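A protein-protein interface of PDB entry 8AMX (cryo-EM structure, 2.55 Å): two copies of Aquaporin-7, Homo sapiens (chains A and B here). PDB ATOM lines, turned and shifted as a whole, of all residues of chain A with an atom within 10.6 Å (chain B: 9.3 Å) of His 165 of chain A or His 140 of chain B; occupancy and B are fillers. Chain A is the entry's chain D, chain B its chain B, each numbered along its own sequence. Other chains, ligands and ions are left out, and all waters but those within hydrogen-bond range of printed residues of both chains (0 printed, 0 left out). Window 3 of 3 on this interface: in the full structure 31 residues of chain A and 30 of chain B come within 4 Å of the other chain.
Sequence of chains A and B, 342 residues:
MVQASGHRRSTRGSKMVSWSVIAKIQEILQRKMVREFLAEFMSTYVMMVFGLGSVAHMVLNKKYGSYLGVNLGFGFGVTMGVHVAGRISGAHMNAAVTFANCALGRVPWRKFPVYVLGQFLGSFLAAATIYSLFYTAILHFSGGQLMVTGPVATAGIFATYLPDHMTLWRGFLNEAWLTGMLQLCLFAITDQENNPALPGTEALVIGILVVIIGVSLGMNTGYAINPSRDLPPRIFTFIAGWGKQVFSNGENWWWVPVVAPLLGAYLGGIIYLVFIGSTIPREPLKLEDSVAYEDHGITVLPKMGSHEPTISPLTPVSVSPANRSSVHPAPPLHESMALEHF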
ATOM      1  N   TYR A 161      10.492  11.238 -12.994  1.00  0.00           N
ATOM      2  CA  TYR A 161      11.698  10.998 -12.219  1.00  0.00           C
ATOM      3  C   TYR A 161      11.704   9.567 -11.704  1.00  0.00           C
ATOM      4  O   TYR A 161      10.656   8.990 -11.410  1.00  0.00           O
ATOM      5  CB  TYR A 161      11.818  11.993 -11.056  1.00  0.00           C
ATOM      6  CG  TYR A 161      12.028  13.412 -11.528  1.00  0.00           C
ATOM      7  CD1 TYR A 161      10.950  14.246 -11.779  1.00  0.00           C
ATOM      8  CD2 TYR A 161      13.303  13.905 -11.755  1.00  0.00           C
ATOM      9  CE1 TYR A 161      11.138  15.526 -12.225  1.00  0.00           C
ATOM     10  CE2 TYR A 161      13.497  15.187 -12.200  1.00  0.00           C
ATOM     11  CZ  TYR A 161      12.410  15.993 -12.436  1.00  0.00           C
ATOM     12  OH  TYR A 161      12.600  17.274 -12.879  1.00  0.00           O
ATOM     13  N   LEU A 162      12.901   9.007 -11.596  1.00  0.00           N
ATOM     14  CA  LEU A 162      13.055   7.595 -11.266  1.00  0.00           C
ATOM     15  C   LEU A 162      12.676   7.336  -9.811  1.00  0.00           C
ATOM     16  O   LEU A 162      13.125   8.065  -8.920  1.00  0.00           O
ATOM     17  CB  LEU A 162      14.496   7.170 -11.529  1.00  0.00           C
ATOM     18  CG  LEU A 162      14.798   5.716 -11.882  1.00  0.00           C
ATOM     19  CD1 LEU A 162      13.919   5.251 -13.019  1.00  0.00           C
ATOM     20  CD2 LEU A 162      16.258   5.586 -12.256  1.00  0.00           C
ATOM     21  N   PRO A 163      11.862   6.311  -9.527  1.00  0.00           N
ATOM     22  CA  PRO A 163      11.480   6.020  -8.136  1.00  0.00           C
ATOM     23  C   PRO A 163      12.635   5.536  -7.268  1.00  0.00           C
ATOM     24  O   PRO A 163      13.783   5.468  -7.720  1.00  0.00           O
ATOM     25  CB  PRO A 163      10.411   4.930  -8.290  1.00  0.00           C
ATOM     26  CG  PRO A 163       9.904   5.087  -9.678  1.00  0.00           C
ATOM     27  CD  PRO A 163      11.085   5.512 -10.487  1.00  0.00           C
ATOM     28  N   ASP A 164      12.334   5.195  -6.012  1.00  0.00           N
ATOM     29  CA  ASP A 164      13.387   4.948  -5.027  1.00  0.00           C
ATOM     30  C   ASP A 164      14.154   3.660  -5.310  1.00  0.00           C
ATOM     31  O   ASP A 164      15.391   3.651  -5.304  1.00  0.00           O
ATOM     32  CB  ASP A 164      12.789   4.911  -3.621  1.00  0.00           C
ATOM     33  CG  ASP A 164      12.535   6.294  -3.057  1.00  0.00           C
ATOM     34  OD1 ASP A 164      13.336   7.209  -3.342  1.00  0.00           O
ATOM     35  OD2 ASP A 164      11.535   6.467  -2.329  1.00  0.00           O
ATOM     36  N   HIS A 165      13.447   2.563  -5.558  1.00  0.00           N
ATOM     37  CA  HIS A 165      14.079   1.250  -5.605  1.00  0.00           C
ATOM     38  C   HIS A 165      14.540   0.838  -6.997  1.00  0.00           C
ATOM     39  O   HIS A 165      15.096  -0.253  -7.146  1.00  0.00           O
ATOM     40  CB  HIS A 165      13.119   0.186  -5.053  1.00  0.00           C
ATOM     41  CG  HIS A 165      11.774   0.184  -5.710  1.00  0.00           C
ATOM     42  ND1 HIS A 165      11.607   0.020  -7.068  1.00  0.00           N
ATOM     43  CD2 HIS A 165      10.531   0.328  -5.194  1.00  0.00           C
ATOM     44  CE1 HIS A 165      10.320   0.066  -7.362  1.00  0.00           C
ATOM     45  NE2 HIS A 165       9.645   0.251  -6.241  1.00  0.00           N
ATOM     46  N   MET A 166      14.339   1.672  -8.010  1.00  0.00           N
ATOM     47  CA  MET A 166      14.597   1.295  -9.392  1.00  0.00           C
ATOM     48  C   MET A 166      15.921   1.877  -9.872  1.00  0.00           C
ATOM     49  O   MET A 166      16.305   2.980  -9.475  1.00  0.00           O
ATOM     50  CB  MET A 166      13.443   1.758 -10.288  1.00  0.00           C
ATOM     51  CG  MET A 166      13.641   1.491 -11.767  1.00  0.00           C
ATOM     52  SD  MET A 166      12.164   0.895 -12.592  1.00  0.00           S
ATOM     53  CE  MET A 166      12.038  -0.735 -11.886  1.00  0.00           C
ATOM     54  N   THR A 167      16.622   1.121 -10.716  1.00  0.00           N
ATOM     55  CA  THR A 167      17.877   1.563 -11.301  1.00  0.00           C
ATOM     56  C   THR A 167      17.645   2.124 -12.705  1.00  0.00           C
ATOM     57  O   THR A 167      16.519   2.199 -13.197  1.00  0.00           O
ATOM     58  CB  THR A 167      18.891   0.421 -11.321  1.00  0.00           C
ATOM     59  OG1 THR A 167      18.418  -0.635 -12.162  1.00  0.00           O
ATOM     60  CG2 THR A 167      19.098  -0.122  -9.926  1.00  0.00           C
ATOM     61  N   LEU A 168      18.733   2.532 -13.360  1.00  0.00           N
ATOM     62  CA  LEU A 168      18.622   3.214 -14.646  1.00  0.00           C
ATOM     63  C   LEU A 168      18.260   2.250 -15.773  1.00  0.00           C
ATOM     64  O   LEU A 168      17.394   2.550 -16.602  1.00  0.00           O
ATOM     65  CB  LEU A 168      19.930   3.937 -14.961  1.00  0.00           C
ATOM     66  CG  LEU A 168      19.929   4.920 -16.130  1.00  0.00           C
ATOM     67  CD1 LEU A 168      19.723   6.339 -15.635  1.00  0.00           C
ATOM     68  CD2 LEU A 168      21.204   4.806 -16.933  1.00  0.00           C
ATOM     69  N   TRP A 169      18.910   1.086 -15.824  1.00  0.00           N
ATOM     70  CA  TRP A 169      18.673   0.157 -16.922  1.00  0.00           C
ATOM     71  C   TRP A 169      17.365  -0.607 -16.763  1.00  0.00           C
ATOM     72  O   TRP A 169      16.755  -0.999 -17.766  1.00  0.00           O
ATOM     73  CB  TRP A 169      19.864  -0.788 -17.063  1.00  0.00           C
ATOM     74  CG  TRP A 169      21.109  -0.049 -17.445  1.00  0.00           C
ATOM     75  CD1 TRP A 169      22.165   0.244 -16.640  1.00  0.00           C
ATOM     76  CD2 TRP A 169      21.408   0.528 -18.725  1.00  0.00           C
ATOM     77  NE1 TRP A 169      23.112   0.952 -17.337  1.00  0.00           N
ATOM     78  CE2 TRP A 169      22.671   1.141 -18.619  1.00  0.00           C
ATOM     79  CE3 TRP A 169      20.735   0.581 -19.949  1.00  0.00           C
ATOM     80  CZ2 TRP A 169      23.273   1.795 -19.688  1.00  0.00           C
ATOM     81  CZ3 TRP A 169      21.336   1.228 -21.009  1.00  0.00           C
ATOM     82  CH2 TRP A 169      22.590   1.826 -20.873  1.00  0.00           C
ATOM     83  N   ARG A 170      16.897  -0.796 -15.529  1.00  0.00           N
ATOM     84  CA  ARG A 170      15.538  -1.285 -15.327  1.00  0.00           C
ATOM     85  C   ARG A 170      14.515  -0.318 -15.914  1.00  0.00           C
ATOM     86  O   ARG A 170      13.558  -0.737 -16.579  1.00  0.00           O
ATOM     87  CB  ARG A 170      15.275  -1.500 -13.838  1.00  0.00           C
ATOM     88  CG  ARG A 170      16.042  -2.650 -13.223  1.00  0.00           C
ATOM     89  CD  ARG A 170      15.420  -3.982 -13.585  1.00  0.00           C
ATOM     90  NE  ARG A 170      16.173  -5.098 -13.025  1.00  0.00           N
ATOM     91  CZ  ARG A 170      15.877  -6.374 -13.220  1.00  0.00           C
ATOM     92  NH1 ARG A 170      14.834  -6.738 -13.944  1.00  0.00           N
ATOM     93  NH2 ARG A 170      16.649  -7.309 -12.676  1.00  0.00           N
ATOM     94  N   GLY A 171      14.708   0.982 -15.689  1.00  0.00           N
ATOM     95  CA  GLY A 171      13.824   1.968 -16.284  1.00  0.00           C
ATOM     96  C   GLY A 171      13.921   2.010 -17.796  1.00  0.00           C
ATOM     97  O   GLY A 171      12.921   2.229 -18.484  1.00  0.00           O
ATOM     98  N   ASN A 174      11.847  -0.825 -18.990  1.00  0.00           N
ATOM     99  CA  ASN A 174      10.433  -0.499 -18.826  1.00  0.00           C
ATOM    100  C   ASN A 174       9.935   0.412 -19.941  1.00  0.00           C
ATOM    101  O   ASN A 174       8.880   0.162 -20.541  1.00  0.00           O
ATOM    102  CB  ASN A 174      10.208   0.158 -17.467  1.00  0.00           C
ATOM    103  CG  ASN A 174       9.761  -0.819 -16.414  1.00  0.00           C
ATOM    104  OD1 ASN A 174       8.573  -0.930 -16.128  1.00  0.00           O
ATOM    105  ND2 ASN A 174      10.707  -1.534 -15.829  1.00  0.00           N
ATOM    106  N   GLY A 218       2.278   1.623 -15.223  1.00  0.00           N
ATOM    107  CA  GLY A 218       2.741   2.992 -15.143  1.00  0.00           C
ATOM    108  C   GLY A 218       3.393   3.468 -13.865  1.00  0.00           C
ATOM    109  O   GLY A 218       3.645   4.673 -13.737  1.00  0.00           O
ATOM    110  N   MET A 219       3.702   2.587 -12.915  1.00  0.00           N
ATOM    111  CA  MET A 219       4.272   3.046 -11.655  1.00  0.00           C
ATOM    112  C   MET A 219       5.783   2.877 -11.563  1.00  0.00           C
ATOM    113  O   MET A 219       6.404   3.510 -10.703  1.00  0.00           O
ATOM    114  CB  MET A 219       3.619   2.326 -10.470  1.00  0.00           C
ATOM    115  CG  MET A 219       4.182   0.949 -10.171  1.00  0.00           C
ATOM    116  SD  MET A 219       3.363   0.179  -8.765  1.00  0.00           S
ATOM    117  CE  MET A 219       4.420  -1.229  -8.493  1.00  0.00           C
ATOM    118  N   ASN A 220       6.390   2.058 -12.418  1.00  0.00           N
ATOM    119  CA  ASN A 220       7.830   1.838 -12.326  1.00  0.00           C
ATOM    120  C   ASN A 220       8.639   3.002 -12.884  1.00  0.00           C
ATOM    121  O   ASN A 220       9.742   3.263 -12.397  1.00  0.00           O
ATOM    122  CB  ASN A 220       8.215   0.544 -13.042  1.00  0.00           C
ATOM    123  CG  ASN A 220       7.587  -0.678 -12.414  1.00  0.00           C
ATOM    124  OD1 ASN A 220       7.849  -0.999 -11.258  1.00  0.00           O
ATOM    125  ND2 ASN A 220       6.759  -1.373 -13.177  1.00  0.00           N
ATOM    126  N   THR A 221       8.134   3.700 -13.902  1.00  0.00           N
ATOM    127  CA  THR A 221       8.848   4.831 -14.478  1.00  0.00           C
ATOM    128  C   THR A 221       7.993   6.076 -14.659  1.00  0.00           C
ATOM    129  O   THR A 221       8.533   7.122 -15.033  1.00  0.00           O
ATOM    130  CB  THR A 221       9.458   4.460 -15.843  1.00  0.00           C
ATOM    131  OG1 THR A 221       8.434   3.972 -16.718  1.00  0.00           O
ATOM    132  CG2 THR A 221      10.537   3.409 -15.690  1.00  0.00           C
ATOM    133  N   GLY A 222       6.691   6.008 -14.392  1.00  0.00           N
ATOM    134  CA  GLY A 222       5.796   7.096 -14.723  1.00  0.00           C
ATOM    135  C   GLY A 222       5.267   7.072 -16.139  1.00  0.00           C
ATOM    136  O   GLY A 222       4.570   8.011 -16.534  1.00  0.00           O
ATOM    137  N   GLY A 250      18.660  11.437 -10.358  1.00  0.00           N
ATOM    138  CA  GLY A 250      18.615  10.040 -10.755  1.00  0.00           C
ATOM    139  C   GLY A 250      19.729   9.609 -11.683  1.00  0.00           C
ATOM    140  O   GLY A 250      19.467   8.907 -12.665  1.00  0.00           O
ATOM    141  N   GLU A 251      20.965  10.005 -11.384  1.00  0.00           N
ATOM    142  CA  GLU A 251      22.162   9.743 -12.191  1.00  0.00           C
ATOM    143  C   GLU A 251      21.899   9.949 -13.684  1.00  0.00           C
ATOM    144  O   GLU A 251      22.069   9.055 -14.512  1.00  0.00           O
ATOM    145  CB  GLU A 251      22.752   8.352 -11.907  1.00  0.00           C
ATOM    146  CG  GLU A 251      21.835   7.150 -12.089  1.00  0.00           C
ATOM    147  CD  GLU A 251      22.537   5.831 -11.844  1.00  0.00           C
ATOM    148  OE1 GLU A 251      23.778   5.785 -11.962  1.00  0.00           O
ATOM    149  OE2 GLU A 251      21.847   4.837 -11.532  1.00  0.00           O
ATOM    150  N   LEU B  60       1.466  -4.633  -4.807  1.00  0.00           N
ATOM    151  CA  LEU B  60       2.712  -4.045  -4.320  1.00  0.00           C
ATOM    152  C   LEU B  60       2.524  -2.639  -3.757  1.00  0.00           C
ATOM    153  O   LEU B  60       3.131  -2.297  -2.739  1.00  0.00           O
ATOM    154  CB  LEU B  60       3.754  -4.035  -5.437  1.00  0.00           C
ATOM    155  CG  LEU B  60       4.170  -5.409  -5.959  1.00  0.00           C
ATOM    156  CD1 LEU B  60       5.044  -5.282  -7.194  1.00  0.00           C
ATOM    157  CD2 LEU B  60       4.872  -6.201  -4.873  1.00  0.00           C
ATOM    158  N   ASN B  61       1.710  -1.806  -4.399  1.00  0.00           N
ATOM    159  CA  ASN B  61       1.618  -0.389  -4.064  1.00  0.00           C
ATOM    160  C   ASN B  61       0.195  -0.038  -3.659  1.00  0.00           C
ATOM    161  O   ASN B  61      -0.751  -0.310  -4.402  1.00  0.00           O
ATOM    162  CB  ASN B  61       2.054   0.473  -5.250  1.00  0.00           C
ATOM    163  CG  ASN B  61       2.728   1.755  -4.823  1.00  0.00           C
ATOM    164  OD1 ASN B  61       3.256   1.857  -3.719  1.00  0.00           O
ATOM    165  ND2 ASN B  61       2.722   2.745  -5.705  1.00  0.00           N
ATOM    166  N   LEU B 133       9.716  -7.032 -15.330  1.00  0.00           N
ATOM    167  CA  LEU B 133       9.469  -5.595 -15.233  1.00  0.00           C
ATOM    168  C   LEU B 133       9.290  -5.112 -13.797  1.00  0.00           C
ATOM    169  O   LEU B 133       9.580  -3.949 -13.507  1.00  0.00           O
ATOM    170  CB  LEU B 133       8.237  -5.203 -16.051  1.00  0.00           C
ATOM    171  CG  LEU B 133       8.299  -5.256 -17.579  1.00  0.00           C
ATOM    172  CD1 LEU B 133       7.006  -4.732 -18.163  1.00  0.00           C
ATOM    173  CD2 LEU B 133       9.481  -4.488 -18.127  1.00  0.00           C
ATOM    174  N   PHE B 134       8.805  -5.966 -12.895  1.00  0.00           N
ATOM    175  CA  PHE B 134       8.474  -5.569 -11.531  1.00  0.00           C
ATOM    176  C   PHE B 134       9.427  -6.161 -10.498  1.00  0.00           C
ATOM    177  O   PHE B 134       9.063  -6.274  -9.327  1.00  0.00           O
ATOM    178  CB  PHE B 134       7.039  -5.977 -11.188  1.00  0.00           C
ATOM    179  CG  PHE B 134       5.981  -5.128 -11.832  1.00  0.00           C
ATOM    180  CD1 PHE B 134       5.608  -5.333 -13.148  1.00  0.00           C
ATOM    181  CD2 PHE B 134       5.334  -4.143 -11.109  1.00  0.00           C
ATOM    182  CE1 PHE B 134       4.632  -4.562 -13.733  1.00  0.00           C
ATOM    183  CE2 PHE B 134       4.355  -3.369 -11.690  1.00  0.00           C
ATOM    184  CZ  PHE B 134       4.004  -3.580 -13.004  1.00  0.00           C
ATOM    185  N   TYR B 135      10.642  -6.529 -10.904  1.00  0.00           N
ATOM    186  CA  TYR B 135      11.523  -7.318 -10.046  1.00  0.00           C
ATOM    187  C   TYR B 135      11.903  -6.569  -8.771  1.00  0.00           C
ATOM    188  O   TYR B 135      11.761  -7.095  -7.655  1.00  0.00           O
ATOM    189  CB  TYR B 135      12.768  -7.713 -10.838  1.00  0.00           C
ATOM    190  CG  TYR B 135      13.764  -8.541 -10.072  1.00  0.00           C
ATOM    191  CD1 TYR B 135      13.556  -9.896  -9.866  1.00  0.00           C
ATOM    192  CD2 TYR B 135      14.922  -7.970  -9.564  1.00  0.00           C
ATOM    193  CE1 TYR B 135      14.465 -10.656  -9.168  1.00  0.00           C
ATOM    194  CE2 TYR B 135      15.835  -8.720  -8.868  1.00  0.00           C
ATOM    195  CZ  TYR B 135      15.604 -10.062  -8.672  1.00  0.00           C
ATOM    196  OH  TYR B 135      16.520 -10.813  -7.974  1.00  0.00           O
ATOM    197  N   THR B 136      12.388  -5.333  -8.914  1.00  0.00           N
ATOM    198  CA  THR B 136      12.855  -4.582  -7.753  1.00  0.00           C
ATOM    199  C   THR B 136      11.717  -4.272  -6.794  1.00  0.00           C
ATOM    200  O   THR B 136      11.908  -4.288  -5.575  1.00  0.00           O
ATOM    201  CB  THR B 136      13.551  -3.294  -8.193  1.00  0.00           C
ATOM    202  OG1 THR B 136      12.666  -2.516  -9.003  1.00  0.00           O
ATOM    203  CG2 THR B 136      14.804  -3.607  -8.982  1.00  0.00           C
ATOM    204  N   ALA B 137      10.528  -3.973  -7.319  1.00  0.00           N
ATOM    205  CA  ALA B 137       9.383  -3.713  -6.452  1.00  0.00           C
ATOM    206  C   ALA B 137       8.993  -4.955  -5.661  1.00  0.00           C
ATOM    207  O   ALA B 137       8.653  -4.863  -4.478  1.00  0.00           O
ATOM    208  CB  ALA B 137       8.203  -3.206  -7.275  1.00  0.00           C
ATOM    209  N   ILE B 138       9.039  -6.125  -6.295  1.00  0.00           N
ATOM    210  CA  ILE B 138       8.731  -7.369  -5.596  1.00  0.00           C
ATOM    211  C   ILE B 138       9.728  -7.607  -4.470  1.00  0.00           C
ATOM    212  O   ILE B 138       9.347  -7.927  -3.335  1.00  0.00           O
ATOM    213  CB  ILE B 138       8.701  -8.546  -6.589  1.00  0.00           C
ATOM    214  CG1 ILE B 138       7.488  -8.431  -7.512  1.00  0.00           C
ATOM    215  CG2 ILE B 138       8.695  -9.872  -5.855  1.00  0.00           C
ATOM    216  CD1 ILE B 138       7.532  -9.355  -8.698  1.00  0.00           C
ATOM    217  N   LEU B 139      11.021  -7.438  -4.761  1.00  0.00           N
ATOM    218  CA  LEU B 139      12.035  -7.659  -3.730  1.00  0.00           C
ATOM    219  C   LEU B 139      11.922  -6.643  -2.597  1.00  0.00           C
ATOM    220  O   LEU B 139      12.080  -6.994  -1.424  1.00  0.00           O
ATOM    221  CB  LEU B 139      13.432  -7.626  -4.339  1.00  0.00           C
ATOM    222  CG  LEU B 139      13.822  -8.874  -5.128  1.00  0.00           C
ATOM    223  CD1 LEU B 139      15.316  -8.907  -5.346  1.00  0.00           C
ATOM    224  CD2 LEU B 139      13.353 -10.120  -4.410  1.00  0.00           C
ATOM    225  N   HIS B 140      11.657  -5.379  -2.925  1.00  0.00           N
ATOM    226  CA  HIS B 140      11.511  -4.360  -1.893  1.00  0.00           C
ATOM    227  C   HIS B 140      10.284  -4.612  -1.028  1.00  0.00           C
ATOM    228  O   HIS B 140      10.324  -4.394   0.188  1.00  0.00           O
ATOM    229  CB  HIS B 140      11.443  -2.975  -2.536  1.00  0.00           C
ATOM    230  CG  HIS B 140      11.210  -1.865  -1.559  1.00  0.00           C
ATOM    231  ND1 HIS B 140      11.819  -1.821  -0.324  1.00  0.00           N
ATOM    232  CD2 HIS B 140      10.439  -0.756  -1.638  1.00  0.00           C
ATOM    233  CE1 HIS B 140      11.431  -0.734   0.318  1.00  0.00           C
ATOM    234  NE2 HIS B 140      10.593  -0.070  -0.457  1.00  0.00           N
ATOM    235  N   PHE B 141       9.182  -5.061  -1.632  1.00  0.00           N
ATOM    236  CA  PHE B 141       7.969  -5.328  -0.867  1.00  0.00           C
ATOM    237  C   PHE B 141       8.150  -6.522   0.062  1.00  0.00           C
ATOM    238  O   PHE B 141       7.788  -6.463   1.241  1.00  0.00           O
ATOM    239  CB  PHE B 141       6.799  -5.557  -1.828  1.00  0.00           C
ATOM    240  CG  PHE B 141       5.530  -6.010  -1.162  1.00  0.00           C
ATOM    241  CD1 PHE B 141       4.652  -5.093  -0.619  1.00  0.00           C
ATOM    242  CD2 PHE B 141       5.202  -7.353  -1.107  1.00  0.00           C
ATOM    243  CE1 PHE B 141       3.486  -5.507  -0.016  1.00  0.00           C
ATOM    244  CE2 PHE B 141       4.036  -7.769  -0.507  1.00  0.00           C
ATOM    245  CZ  PHE B 141       3.179  -6.844   0.039  1.00  0.00           C
ATOM    246  N   SER B 142       8.710  -7.614  -0.448  1.00  0.00           N
ATOM    247  CA  SER B 142       8.721  -8.853   0.315  1.00  0.00           C
ATOM    248  C   SER B 142       9.931  -8.997   1.227  1.00  0.00           C
ATOM    249  O   SER B 142       9.984  -9.950   2.008  1.00  0.00           O
ATOM    250  CB  SER B 142       8.653 -10.053  -0.634  1.00  0.00           C
ATOM    251  OG  SER B 142       9.775 -10.095  -1.494  1.00  0.00           O
ATOM    252  N   GLY B 143      10.891  -8.077   1.160  1.00  0.00           N
ATOM    253  CA  GLY B 143      12.109  -8.213   1.930  1.00  0.00           C
ATOM    254  C   GLY B 143      13.063  -9.258   1.408  1.00  0.00           C
ATOM    255  O   GLY B 143      13.914  -9.736   2.160  1.00  0.00           O
ATOM    256  N   GLY B 144      12.947  -9.628   0.136  1.00  0.00           N
ATOM    257  CA  GLY B 144      13.779 -10.652  -0.458  1.00  0.00           C
ATOM    258  C   GLY B 144      13.244 -12.064  -0.360  1.00  0.00           C
ATOM    259  O   GLY B 144      13.882 -12.984  -0.884  1.00  0.00           O
ATOM    260  N   GLN B 145      12.095 -12.267   0.277  1.00  0.00           N
ATOM    261  CA  GLN B 145      11.539 -13.595   0.516  1.00  0.00           C
ATOM    262  C   GLN B 145      10.375 -13.832  -0.434  1.00  0.00           C
ATOM    263  O   GLN B 145       9.427 -13.043  -0.464  1.00  0.00           O
ATOM    264  CB  GLN B 145      11.077 -13.737   1.965  1.00  0.00           C
ATOM    265  CG  GLN B 145      12.119 -13.335   2.991  1.00  0.00           C
ATOM    266  CD  GLN B 145      13.365 -14.182   2.907  1.00  0.00           C
ATOM    267  OE1 GLN B 145      13.297 -15.409   2.935  1.00  0.00           O
ATOM    268  NE2 GLN B 145      14.515 -13.531   2.795  1.00  0.00           N
ATOM    269  N   LEU B 146      10.440 -14.919  -1.198  1.00  0.00           N
ATOM    270  CA  LEU B 146       9.365 -15.285  -2.116  1.00  0.00           C
ATOM    271  C   LEU B 146       8.428 -16.241  -1.386  1.00  0.00           C
ATOM    272  O   LEU B 146       8.701 -17.437  -1.277  1.00  0.00           O
ATOM    273  CB  LEU B 146       9.932 -15.895  -3.392  1.00  0.00           C
ATOM    274  CG  LEU B 146      10.882 -15.002  -4.196  1.00  0.00           C
ATOM    275  CD1 LEU B 146      11.244 -15.649  -5.513  1.00  0.00           C
ATOM    276  CD2 LEU B 146      10.292 -13.623  -4.424  1.00  0.00           C
ATOM    277  N   VAL B 152       3.311 -10.892   3.504  1.00  0.00           N
ATOM    278  CA  VAL B 152       4.096 -10.386   2.380  1.00  0.00           C
ATOM    279  C   VAL B 152       4.133 -11.414   1.256  1.00  0.00           C
ATOM    280  O   VAL B 152       5.138 -11.536   0.547  1.00  0.00           O
ATOM    281  CB  VAL B 152       5.522  -9.994   2.812  1.00  0.00           C
ATOM    282  CG1 VAL B 152       5.510  -8.662   3.534  1.00  0.00           C
ATOM    283  CG2 VAL B 152       6.138 -11.074   3.682  1.00  0.00           C
ATOM    284  N   THR B 154       3.623 -12.989  -2.308  1.00  0.00           N
ATOM    285  CA  THR B 154       3.657 -12.428  -3.650  1.00  0.00           C
ATOM    286  C   THR B 154       3.314 -13.424  -4.747  1.00  0.00           C
ATOM    287  O   THR B 154       3.350 -13.052  -5.922  1.00  0.00           O
ATOM    288  CB  THR B 154       5.038 -11.825  -3.959  1.00  0.00           C
ATOM    289  OG1 THR B 154       6.068 -12.714  -3.513  1.00  0.00           O
ATOM    290  CG2 THR B 154       5.203 -10.475  -3.290  1.00  0.00           C
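No position is printed for both chains.
Of the 10 pairs that touch across the chains among the printed residues, none has its exchanged pair printed and touching as well.
Hydrophobic or aromatic side chains of chain B within 4 Å of the printed part of chain A: Leu 133, Phe 134, Tyr 135, Ala 137 and His 140.
Along chain B the printed residues that touch a printed residue of chain A span positions 61 to 140.
Of the 19 printed residues of chain A, 6 touch a printed residue of chain B.
Among the printed residues, 10 pairs touch across the chains.
Among the printed residues, no Asp or Glu carboxylate lies within 4 Å of a Lys or Arg side-chain nitrogen of the other chain.
Of chain A, only His 165 (3.7 Å) comes within 4 Å of His 140 of chain B.
No residue of chain A comes within 4 Å of Leu 139 of chain B.
No residue of chain A comes within 4 Å of Ser 142 of chain B.
Printed residues of chain A within 4 Å of Leu 133 of chain B: Asn 174 and Asn 220.
Of the printed residues of chain A, Tyr 135 of chain B touches Arg 170.
Of the printed residues of chain A, Phe 134 of chain B touches Met 219 (3.8 Å) and Asn 220 (3.5 Å).
Printed residues of chain B within 4 Å of Met 166 of chain A: Thr 136 (3.4 Å).
Printed residues of chain B within 4 Å of Asn 174 of chain A: Leu 133 (3.5 Å).
Gln 145 of chain B touches none of the printed residues of chain A.
The nearest residue of chain B that does not touch His 165 of chain A is Ile 138 of chain B (6.4 Å).
A ring nitrogen (ND1) of His 165 of chain A sits at hydrogen-bond distance from the side-chain hydroxyl (OG1) of Thr 136 of chain B (3.4 Å).
NE2 of His 165 of chain A touches CB of Ala 137 of chain B (3.9 Å).
CD2 of His 165 of chain A touches CD2 of His 140 of chain B, 3.7 Å away.
Met 166 of chain A touches Thr 136 of chain B (CE to OG1, 3.4 Å).
CD2 of Tyr 135 of chain B touches NH2 of Arg 170 of chain A, 3.6 Å away.
ND2 of Asn 174 of chain A touches O of Leu 133 of chain B, at 3.5 Å.
Asn 61 of chain B touches Met 219 of chain A (CB to SD, 3.8 Å).
CE2 of Phe 134 of chain B touches CE of Met 219 of chain A, at 3.8 Å.
ND2 of Asn 220 of chain A touches O of Leu 133 of chain B, at 3.8 Å.
Asn 220 of chain A touches Phe 134 of chain B.
The side-chain amide nitrogen of Asn 174 of chain A sits at hydrogen-bond distance from the backbone carbonyl oxygen of Arg 170 of chain A (3.1 Å).
The side-chain amide oxygen (OD1) of Asn 174 of chain A lies close to the side-chain amide nitrogen (ND2) of Asn 220 of chain A, at 3.5 Å.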
